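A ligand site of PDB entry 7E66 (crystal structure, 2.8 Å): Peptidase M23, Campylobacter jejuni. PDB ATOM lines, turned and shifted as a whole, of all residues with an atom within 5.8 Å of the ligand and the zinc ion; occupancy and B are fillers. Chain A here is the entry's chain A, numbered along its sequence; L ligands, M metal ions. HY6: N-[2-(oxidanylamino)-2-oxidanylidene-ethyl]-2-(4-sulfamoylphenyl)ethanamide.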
ATOM      1  N   GLU A 102      27.202 -21.528   8.783  1.00  0.00           N
ATOM      2  CA  GLU A 102      26.436 -21.067   7.625  1.00  0.00           C
ATOM      3  C   GLU A 102      26.595 -19.557   7.395  1.00  0.00           C
ATOM      4  O   GLU A 102      26.462 -19.075   6.273  1.00  0.00           O
ATOM      5  CB  GLU A 102      24.959 -21.434   7.779  1.00  0.00           C
ATOM      6  CG  GLU A 102      24.704 -22.922   7.643  1.00  0.00           C
ATOM      7  CD  GLU A 102      23.255 -23.319   7.874  1.00  0.00           C
ATOM      8  OE1 GLU A 102      22.469 -22.490   8.382  1.00  0.00           O
ATOM      9  OE2 GLU A 102      22.902 -24.471   7.568  1.00  0.00           O
ATOM     10  N   LEU A 103      26.867 -18.834   8.472  1.00  0.00           N
ATOM     11  CA  LEU A 103      27.208 -17.420   8.406  1.00  0.00           C
ATOM     12  C   LEU A 103      28.545 -17.209   7.710  1.00  0.00           C
ATOM     13  O   LEU A 103      28.659 -16.385   6.798  1.00  0.00           O
ATOM     14  CB  LEU A 103      27.262 -16.834   9.819  1.00  0.00           C
ATOM     15  CG  LEU A 103      27.604 -15.347   9.930  1.00  0.00           C
ATOM     16  CD1 LEU A 103      26.525 -14.491   9.293  1.00  0.00           C
ATOM     17  CD2 LEU A 103      27.817 -14.953  11.379  1.00  0.00           C
ATOM     18  N   ALA A 106      28.244 -17.829   4.107  1.00  0.00           N
ATOM     19  CA  ALA A 106      27.550 -16.709   3.471  1.00  0.00           C
ATOM     20  C   ALA A 106      28.465 -15.516   3.264  1.00  0.00           C
ATOM     21  O   ALA A 106      28.524 -14.955   2.163  1.00  0.00           O
ATOM     22  CB  ALA A 106      26.345 -16.307   4.297  1.00  0.00           C
ATOM     23  N   TYR A 110      29.321 -13.572  -0.172  1.00  0.00           N
ATOM     24  CA  TYR A 110      28.916 -12.179  -0.403  1.00  0.00           C
ATOM     25  C   TYR A 110      30.068 -11.191  -0.492  1.00  0.00           C
ATOM     26  O   TYR A 110      29.864 -10.038  -0.873  1.00  0.00           O
ATOM     27  CB  TYR A 110      27.930 -11.719   0.675  1.00  0.00           C
ATOM     28  CG  TYR A 110      26.618 -12.448   0.607  1.00  0.00           C
ATOM     29  CD1 TYR A 110      25.952 -12.605  -0.604  1.00  0.00           C
ATOM     30  CD2 TYR A 110      26.031 -12.979   1.755  1.00  0.00           C
ATOM     31  CE1 TYR A 110      24.746 -13.284  -0.678  1.00  0.00           C
ATOM     32  CE2 TYR A 110      24.826 -13.654   1.689  1.00  0.00           C
ATOM     33  CZ  TYR A 110      24.186 -13.803   0.470  1.00  0.00           C
ATOM     34  OH  TYR A 110      22.994 -14.473   0.400  1.00  0.00           O
ATOM     35  N   SER A 133       4.134  -9.533   3.295  1.00  0.00           N
ATOM     36  CA  SER A 133       4.908  -8.852   4.324  1.00  0.00           C
ATOM     37  C   SER A 133       5.998  -7.987   3.676  1.00  0.00           C
ATOM     38  O   SER A 133       6.880  -8.509   3.004  1.00  0.00           O
ATOM     39  CB  SER A 133       5.540  -9.882   5.274  1.00  0.00           C
ATOM     40  OG  SER A 133       6.480  -9.283   6.149  1.00  0.00           O
ATOM     41  N   HIS A 149      12.653  -6.971   8.789  1.00  0.00           N
ATOM     42  CA  HIS A 149      12.480  -7.932   7.711  1.00  0.00           C
ATOM     43  C   HIS A 149      13.462  -7.596   6.596  1.00  0.00           C
ATOM     44  O   HIS A 149      13.352  -6.555   5.951  1.00  0.00           O
ATOM     45  CB  HIS A 149      11.041  -7.885   7.209  1.00  0.00           C
ATOM     46  CG  HIS A 149      10.669  -9.030   6.329  1.00  0.00           C
ATOM     47  ND1 HIS A 149       9.891  -8.867   5.195  1.00  0.00           N
ATOM     48  CD2 HIS A 149      10.970 -10.348   6.394  1.00  0.00           C
ATOM     49  CE1 HIS A 149       9.723 -10.042   4.612  1.00  0.00           C
ATOM     50  NE2 HIS A 149      10.367 -10.954   5.324  1.00  0.00           N
ATOM     51  N   SER A 150      14.428  -8.489   6.372  1.00  0.00           N
ATOM     52  CA  SER A 150      15.516  -8.252   5.422  1.00  0.00           C
ATOM     53  C   SER A 150      15.144  -8.476   3.962  1.00  0.00           C
ATOM     54  O   SER A 150      15.961  -8.265   3.068  1.00  0.00           O
ATOM     55  CB  SER A 150      16.691  -9.163   5.768  1.00  0.00           C
ATOM     56  OG  SER A 150      16.282 -10.512   5.746  1.00  0.00           O
ATOM     57  N   GLY A 151      13.908  -8.923   3.712  1.00  0.00           N
ATOM     58  CA  GLY A 151      13.435  -9.178   2.361  1.00  0.00           C
ATOM     59  C   GLY A 151      11.969  -8.839   2.237  1.00  0.00           C
ATOM     60  O   GLY A 151      11.433  -8.113   3.058  1.00  0.00           O
ATOM     61  N   THR A 152      11.330  -9.372   1.204  1.00  0.00           N
ATOM     62  CA  THR A 152       9.903  -9.160   0.990  1.00  0.00           C
ATOM     63  C   THR A 152       9.242 -10.510   0.773  1.00  0.00           C
ATOM     64  O   THR A 152       9.789 -11.365   0.057  1.00  0.00           O
ATOM     65  CB  THR A 152       9.668  -8.184  -0.199  1.00  0.00           C
ATOM     66  OG1 THR A 152       8.453  -7.456   0.021  1.00  0.00           O
ATOM     67  CG2 THR A 152       9.608  -8.912  -1.543  1.00  0.00           C
ATOM     68  N   ASP A 153       8.081 -10.721   1.384  1.00  0.00           N
ATOM     69  CA  ASP A 153       7.390 -12.001   1.273  1.00  0.00           C
ATOM     70  C   ASP A 153       6.216 -11.924   0.321  1.00  0.00           C
ATOM     71  O   ASP A 153       5.322 -11.099   0.477  1.00  0.00           O
ATOM     72  CB  ASP A 153       6.912 -12.483   2.637  1.00  0.00           C
ATOM     73  CG  ASP A 153       8.051 -12.700   3.618  1.00  0.00           C
ATOM     74  OD1 ASP A 153       9.202 -12.879   3.175  1.00  0.00           O
ATOM     75  OD2 ASP A 153       7.783 -12.694   4.836  1.00  0.00           O
ATOM     76  N   ILE A 172      24.433 -20.747  -3.553  1.00  0.00           N
ATOM     77  CA  ILE A 172      23.883 -21.511  -2.444  1.00  0.00           C
ATOM     78  C   ILE A 172      22.641 -22.237  -2.939  1.00  0.00           C
ATOM     79  O   ILE A 172      21.851 -21.667  -3.697  1.00  0.00           O
ATOM     80  CB  ILE A 172      23.517 -20.595  -1.259  1.00  0.00           C
ATOM     81  CG1 ILE A 172      24.759 -19.816  -0.778  1.00  0.00           C
ATOM     82  CG2 ILE A 172      22.923 -21.413  -0.106  1.00  0.00           C
ATOM     83  CD1 ILE A 172      24.500 -18.851   0.356  1.00  0.00           C
ATOM     84  N   ARG A 176      19.151 -24.397   5.138  1.00  0.00           N
ATOM     85  CA  ARG A 176      19.874 -23.681   6.170  1.00  0.00           C
ATOM     86  C   ARG A 176      18.928 -23.386   7.310  1.00  0.00           C
ATOM     87  O   ARG A 176      17.709 -23.536   7.171  1.00  0.00           O
ATOM     88  CB  ARG A 176      20.451 -22.394   5.611  1.00  0.00           C
ATOM     89  CG  ARG A 176      21.439 -22.639   4.485  1.00  0.00           C
ATOM     90  CD  ARG A 176      22.174 -21.370   4.123  1.00  0.00           C
ATOM     91  NE  ARG A 176      21.283 -20.363   3.551  1.00  0.00           N
ATOM     92  CZ  ARG A 176      21.637 -19.125   3.242  1.00  0.00           C
ATOM     93  NH1 ARG A 176      22.874 -18.707   3.462  1.00  0.00           N
ATOM     94  NH2 ARG A 176      20.740 -18.289   2.731  1.00  0.00           N
ATOM     95  N   PHE A 178      18.039 -20.456   9.453  1.00  0.00           N
ATOM     96  CA  PHE A 178      17.093 -19.352   9.369  1.00  0.00           C
ATOM     97  C   PHE A 178      16.378 -19.293   8.028  1.00  0.00           C
ATOM     98  O   PHE A 178      15.170 -19.056   7.980  1.00  0.00           O
ATOM     99  CB  PHE A 178      17.803 -18.010   9.628  1.00  0.00           C
ATOM    100  CG  PHE A 178      18.237 -17.821  11.051  1.00  0.00           C
ATOM    101  CD1 PHE A 178      17.363 -18.080  12.100  1.00  0.00           C
ATOM    102  CD2 PHE A 178      19.517 -17.367  11.347  1.00  0.00           C
ATOM    103  CE1 PHE A 178      17.764 -17.903  13.410  1.00  0.00           C
ATOM    104  CE2 PHE A 178      19.918 -17.190  12.657  1.00  0.00           C
ATOM    105  CZ  PHE A 178      19.041 -17.458  13.689  1.00  0.00           C
ATOM    106  N   ALA A 179      17.116 -19.538   6.953  1.00  0.00           N
ATOM    107  CA  ALA A 179      16.625 -19.324   5.601  1.00  0.00           C
ATOM    108  C   ALA A 179      15.794 -20.484   5.027  1.00  0.00           C
ATOM    109  O   ALA A 179      15.184 -20.326   3.969  1.00  0.00           O
ATOM    110  CB  ALA A 179      17.786 -19.010   4.671  1.00  0.00           C
ATOM    111  N   VAL A 184      20.572 -18.790  -3.578  1.00  0.00           N
ATOM    112  CA  VAL A 184      21.171 -17.466  -3.743  1.00  0.00           C
ATOM    113  C   VAL A 184      21.933 -17.429  -5.060  1.00  0.00           C
ATOM    114  O   VAL A 184      22.689 -18.345  -5.375  1.00  0.00           O
ATOM    115  CB  VAL A 184      22.111 -17.139  -2.568  1.00  0.00           C
ATOM    116  CG1 VAL A 184      22.775 -15.792  -2.776  1.00  0.00           C
ATOM    117  CG2 VAL A 184      21.346 -17.155  -1.260  1.00  0.00           C
ATOM    118  N   GLN A 194      17.990 -13.679  -3.551  1.00  0.00           N
ATOM    119  CA  GLN A 194      17.808 -14.691  -2.526  1.00  0.00           C
ATOM    120  C   GLN A 194      16.382 -15.215  -2.552  1.00  0.00           C
ATOM    121  O   GLN A 194      15.436 -14.438  -2.678  1.00  0.00           O
ATOM    122  CB  GLN A 194      18.107 -14.088  -1.159  1.00  0.00           C
ATOM    123  CG  GLN A 194      19.472 -13.414  -1.062  1.00  0.00           C
ATOM    124  CD  GLN A 194      19.597 -12.482   0.127  1.00  0.00           C
ATOM    125  OE1 GLN A 194      18.607 -11.923   0.608  1.00  0.00           O
ATOM    126  NE2 GLN A 194      20.817 -12.296   0.619  1.00  0.00           N
ATOM    127  N   TYR A 196      14.037 -17.974  -0.337  1.00  0.00           N
ATOM    128  CA  TYR A 196      14.082 -18.748   0.896  1.00  0.00           C
ATOM    129  C   TYR A 196      12.804 -19.521   1.192  1.00  0.00           C
ATOM    130  O   TYR A 196      11.751 -19.269   0.607  1.00  0.00           O
ATOM    131  CB  TYR A 196      14.391 -17.841   2.091  1.00  0.00           C
ATOM    132  CG  TYR A 196      15.745 -17.150   2.081  1.00  0.00           C
ATOM    133  CD1 TYR A 196      16.761 -17.543   1.213  1.00  0.00           C
ATOM    134  CD2 TYR A 196      16.005 -16.120   2.977  1.00  0.00           C
ATOM    135  CE1 TYR A 196      17.993 -16.913   1.218  1.00  0.00           C
ATOM    136  CE2 TYR A 196      17.239 -15.486   2.991  1.00  0.00           C
ATOM    137  CZ  TYR A 196      18.222 -15.881   2.118  1.00  0.00           C
ATOM    138  OH  TYR A 196      19.445 -15.247   2.122  1.00  0.00           O
ATOM    139  N   HIS A 197      12.932 -20.466   2.136  1.00  0.00           N
ATOM    140  CA  HIS A 197      11.819 -21.264   2.643  1.00  0.00           C
ATOM    141  C   HIS A 197      11.154 -22.081   1.561  1.00  0.00           C
ATOM    142  O   HIS A 197       9.949 -22.316   1.608  1.00  0.00           O
ATOM    143  CB  HIS A 197      10.816 -20.367   3.354  1.00  0.00           C
ATOM    144  CG  HIS A 197      11.454 -19.363   4.248  1.00  0.00           C
ATOM    145  ND1 HIS A 197      12.153 -19.725   5.380  1.00  0.00           N
ATOM    146  CD2 HIS A 197      11.552 -18.020   4.153  1.00  0.00           C
ATOM    147  CE1 HIS A 197      12.628 -18.644   5.959  1.00  0.00           C
ATOM    148  NE2 HIS A 197      12.276 -17.593   5.235  1.00  0.00           N
ATOM    149  N   ARG A 223      10.416 -21.623   8.315  1.00  0.00           N
ATOM    150  CA  ARG A 223       9.517 -20.492   8.448  1.00  0.00           C
ATOM    151  C   ARG A 223       8.463 -20.824   9.494  1.00  0.00           C
ATOM    152  O   ARG A 223       7.821 -21.873   9.419  1.00  0.00           O
ATOM    153  CB  ARG A 223       8.840 -20.203   7.112  1.00  0.00           C
ATOM    154  CG  ARG A 223       8.170 -18.838   7.027  1.00  0.00           C
ATOM    155  CD  ARG A 223       8.086 -18.343   5.588  1.00  0.00           C
ATOM    156  NE  ARG A 223       7.760 -16.928   5.502  1.00  0.00           N
ATOM    157  CZ  ARG A 223       6.540 -16.405   5.677  1.00  0.00           C
ATOM    158  NH1 ARG A 223       5.498 -17.181   5.949  1.00  0.00           N
ATOM    159  NH2 ARG A 223       6.369 -15.090   5.571  1.00  0.00           N
ATOM    160  N   SER A 225       5.789 -18.762  10.296  1.00  0.00           N
ATOM    161  CA  SER A 225       4.485 -18.170   9.980  1.00  0.00           C
ATOM    162  C   SER A 225       3.910 -18.625   8.630  1.00  0.00           C
ATOM    163  O   SER A 225       3.340 -17.826   7.882  1.00  0.00           O
ATOM    164  CB  SER A 225       4.585 -16.645  10.043  1.00  0.00           C
ATOM    165  OG  SER A 225       5.674 -16.176   9.250  1.00  0.00           O
ATOM    166  N   LEU A 229       6.969 -17.175  -0.136  1.00  0.00           N
ATOM    167  CA  LEU A 229       8.295 -16.953  -0.689  1.00  0.00           C
ATOM    168  C   LEU A 229       8.897 -15.710  -0.051  1.00  0.00           C
ATOM    169  O   LEU A 229       8.244 -14.669   0.018  1.00  0.00           O
ATOM    170  CB  LEU A 229       8.280 -16.747  -2.201  1.00  0.00           C
ATOM    171  CG  LEU A 229       9.683 -16.440  -2.762  1.00  0.00           C
ATOM    172  CD1 LEU A 229      10.489 -17.727  -2.916  1.00  0.00           C
ATOM    173  CD2 LEU A 229       9.626 -15.676  -4.067  1.00  0.00           C
ATOM    174  N   HIS A 230      10.150 -15.827   0.381  1.00  0.00           N
ATOM    175  CA  HIS A 230      10.922 -14.687   0.851  1.00  0.00           C
ATOM    176  C   HIS A 230      11.971 -14.368  -0.200  1.00  0.00           C
ATOM    177  O   HIS A 230      12.883 -15.154  -0.446  1.00  0.00           O
ATOM    178  CB  HIS A 230      11.578 -15.031   2.182  1.00  0.00           C
ATOM    179  CG  HIS A 230      12.512 -13.970   2.676  1.00  0.00           C
ATOM    180  ND1 HIS A 230      12.206 -13.155   3.744  1.00  0.00           N
ATOM    181  CD2 HIS A 230      13.743 -13.593   2.265  1.00  0.00           C
ATOM    182  CE1 HIS A 230      13.206 -12.330   3.971  1.00  0.00           C
ATOM    183  NE2 HIS A 230      14.154 -12.571   3.085  1.00  0.00           N
ATOM    184  N   LEU A 234      20.853  -8.666  -2.013  1.00  0.00           N
ATOM    185  CA  LEU A 234      22.046  -8.131  -1.394  1.00  0.00           C
ATOM    186  C   LEU A 234      22.812  -7.362  -2.461  1.00  0.00           C
ATOM    187  O   LEU A 234      23.074  -7.908  -3.539  1.00  0.00           O
ATOM    188  CB  LEU A 234      22.909  -9.237  -0.803  1.00  0.00           C
ATOM    189  CG  LEU A 234      24.016  -8.753   0.146  1.00  0.00           C
ATOM    190  CD1 LEU A 234      24.233  -9.755   1.272  1.00  0.00           C
ATOM    191  CD2 LEU A 234      25.320  -8.495  -0.601  1.00  0.00           C
ATOM    192  N   GLN A 239      21.874  -6.119   2.698  1.00  0.00           N
ATOM    193  CA  GLN A 239      20.472  -6.418   2.391  1.00  0.00           C
ATOM    194  C   GLN A 239      19.781  -5.099   2.096  1.00  0.00           C
ATOM    195  O   GLN A 239      19.924  -4.134   2.851  1.00  0.00           O
ATOM    196  CB  GLN A 239      19.765  -7.085   3.578  1.00  0.00           C
ATOM    197  CG  GLN A 239      20.227  -8.485   3.927  1.00  0.00           C
ATOM    198  CD  GLN A 239      20.139  -9.485   2.775  1.00  0.00           C
ATOM    199  OE1 GLN A 239      20.961 -10.402   2.686  1.00  0.00           O
ATOM    200  NE2 GLN A 239      19.147  -9.322   1.898  1.00  0.00           N
HETATM  201  C5  HY6 L   1      11.645 -14.407   7.247  1.00  0.00           C
HETATM  202  C11 HY6 L   1      18.589 -14.874   6.713  1.00  0.00           C
HETATM  203  N1  HY6 L   1      14.188 -13.775   7.369  1.00  0.00           N
HETATM  204  N2  HY6 L   1      10.932 -14.762   6.038  1.00  0.00           N
HETATM  205  C3  HY6 L   1      13.129 -14.777   7.416  1.00  0.00           C
HETATM  206  C1  HY6 L   1      16.740 -13.216   7.323  1.00  0.00           C
HETATM  207  O1  HY6 L   1      15.806 -15.385   7.401  1.00  0.00           O
HETATM  208  S1  HY6 L   1      21.856 -14.817   4.272  1.00  0.00           S
HETATM  209  C2  HY6 L   1      15.584 -14.218   7.363  1.00  0.00           C
HETATM  210  O2  HY6 L   1      11.074 -13.844   8.119  1.00  0.00           O
HETATM  211  O3  HY6 L   1       9.574 -14.427   5.900  1.00  0.00           O
HETATM  212  O5  HY6 L   1      23.169 -14.060   4.921  1.00  0.00           O
HETATM  213  N7  HY6 L   1      21.682 -14.375   2.625  1.00  0.00           N
HETATM  214  O7  HY6 L   1      22.051 -16.449   4.393  1.00  0.00           O
HETATM  215  C21 HY6 L   1      18.019 -13.617   6.553  1.00  0.00           C
HETATM  216  C31 HY6 L   1      18.649 -12.710   5.698  1.00  0.00           C
HETATM  217  C41 HY6 L   1      19.803 -13.066   5.004  1.00  0.00           C
HETATM  218  C51 HY6 L   1      20.349 -14.328   5.160  1.00  0.00           C
HETATM  219  C61 HY6 L   1      19.730 -15.235   6.023  1.00  0.00           C
HETATM  220 ZN    ZN M   1      10.361 -13.030   4.907  1.00  0.00          ZN
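A nitrogen (N7) of the ligand lies within hydrogen-bond range of the side-chain hydroxyl of Tyr 110 (2.6 Å).
NH1 of Arg 176 lies within hydrogen-bond range of O7 of the ligand (2.6 Å).
The side-chain hydroxyl (OH) of Tyr 196 lies within hydrogen-bond range of a nitrogen (N7) of the ligand.
The side-chain amide nitrogen (NE2) of Gln 194 lies close to a nitrogen (N7) of the ligand (3.0 Å).
An oxygen (O3) of the ligand sits close to the guanidinium group of Arg 223.
A nitrogen (N2) of the ligand sits close to a ring nitrogen (NE2) of His 197, 3.2 Å away.
A ring nitrogen (ND1) of His 149 sits at hydrogen-bond distance from the backbone carbonyl oxygen (O) of Gly 151 (2.7 Å).
The side-chain carboxylate of Asp 153 is in salt-bridge range of the guanidinium group of Arg 223 (2.9 Å).
NH1 of Arg 223 lies within hydrogen-bond range of O of Ser 225, at 3.0 Å.
N of Asp 153 lies within hydrogen-bond range of O of Ser 133 (3.0 Å).
NH2 of Arg 176 is in hydrogen-bond range of OH of Tyr 196, at 3.4 Å.
The side-chain amide nitrogen (NE2) of Gln 194 sits at hydrogen-bond distance from the side-chain amide oxygen (OE1) of Gln 239, 2.8 Å away.
N of His 197 lies within hydrogen-bond range of O of Ala 179.
OH of Tyr 110 sits at hydrogen-bond distance from NE2 of Gln 194, 3.1 Å away.
Ala 106 touches the ligand.
Ser 150 touches the ligand (OG to C1, 3.2 Å).
O of Phe 178 touches O1 of the ligand, 3.8 Å away.
Gln 239 touches the ligand.
Hydrophobic or aromatic side chains that line the ligand: Ala 106, Tyr 110, His 149, Phe 178, Tyr 196, His 197 and His 230.
Of the 24 residues printed, 3 come within 4 Å of the zinc ion.
O3 of the ligand binds the zinc ion (1.9 Å).
OD1 of Asp 153 binds the zinc ion, 2.1 Å away.
The zinc ion is bound by a ring nitrogen (NE2) of His 149 (2.1 Å).
A ring nitrogen (ND1) of His 230 binds the zinc ion.
Slightly farther from the zinc ion lies OD2 of Asp 153 (2.6 Å).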
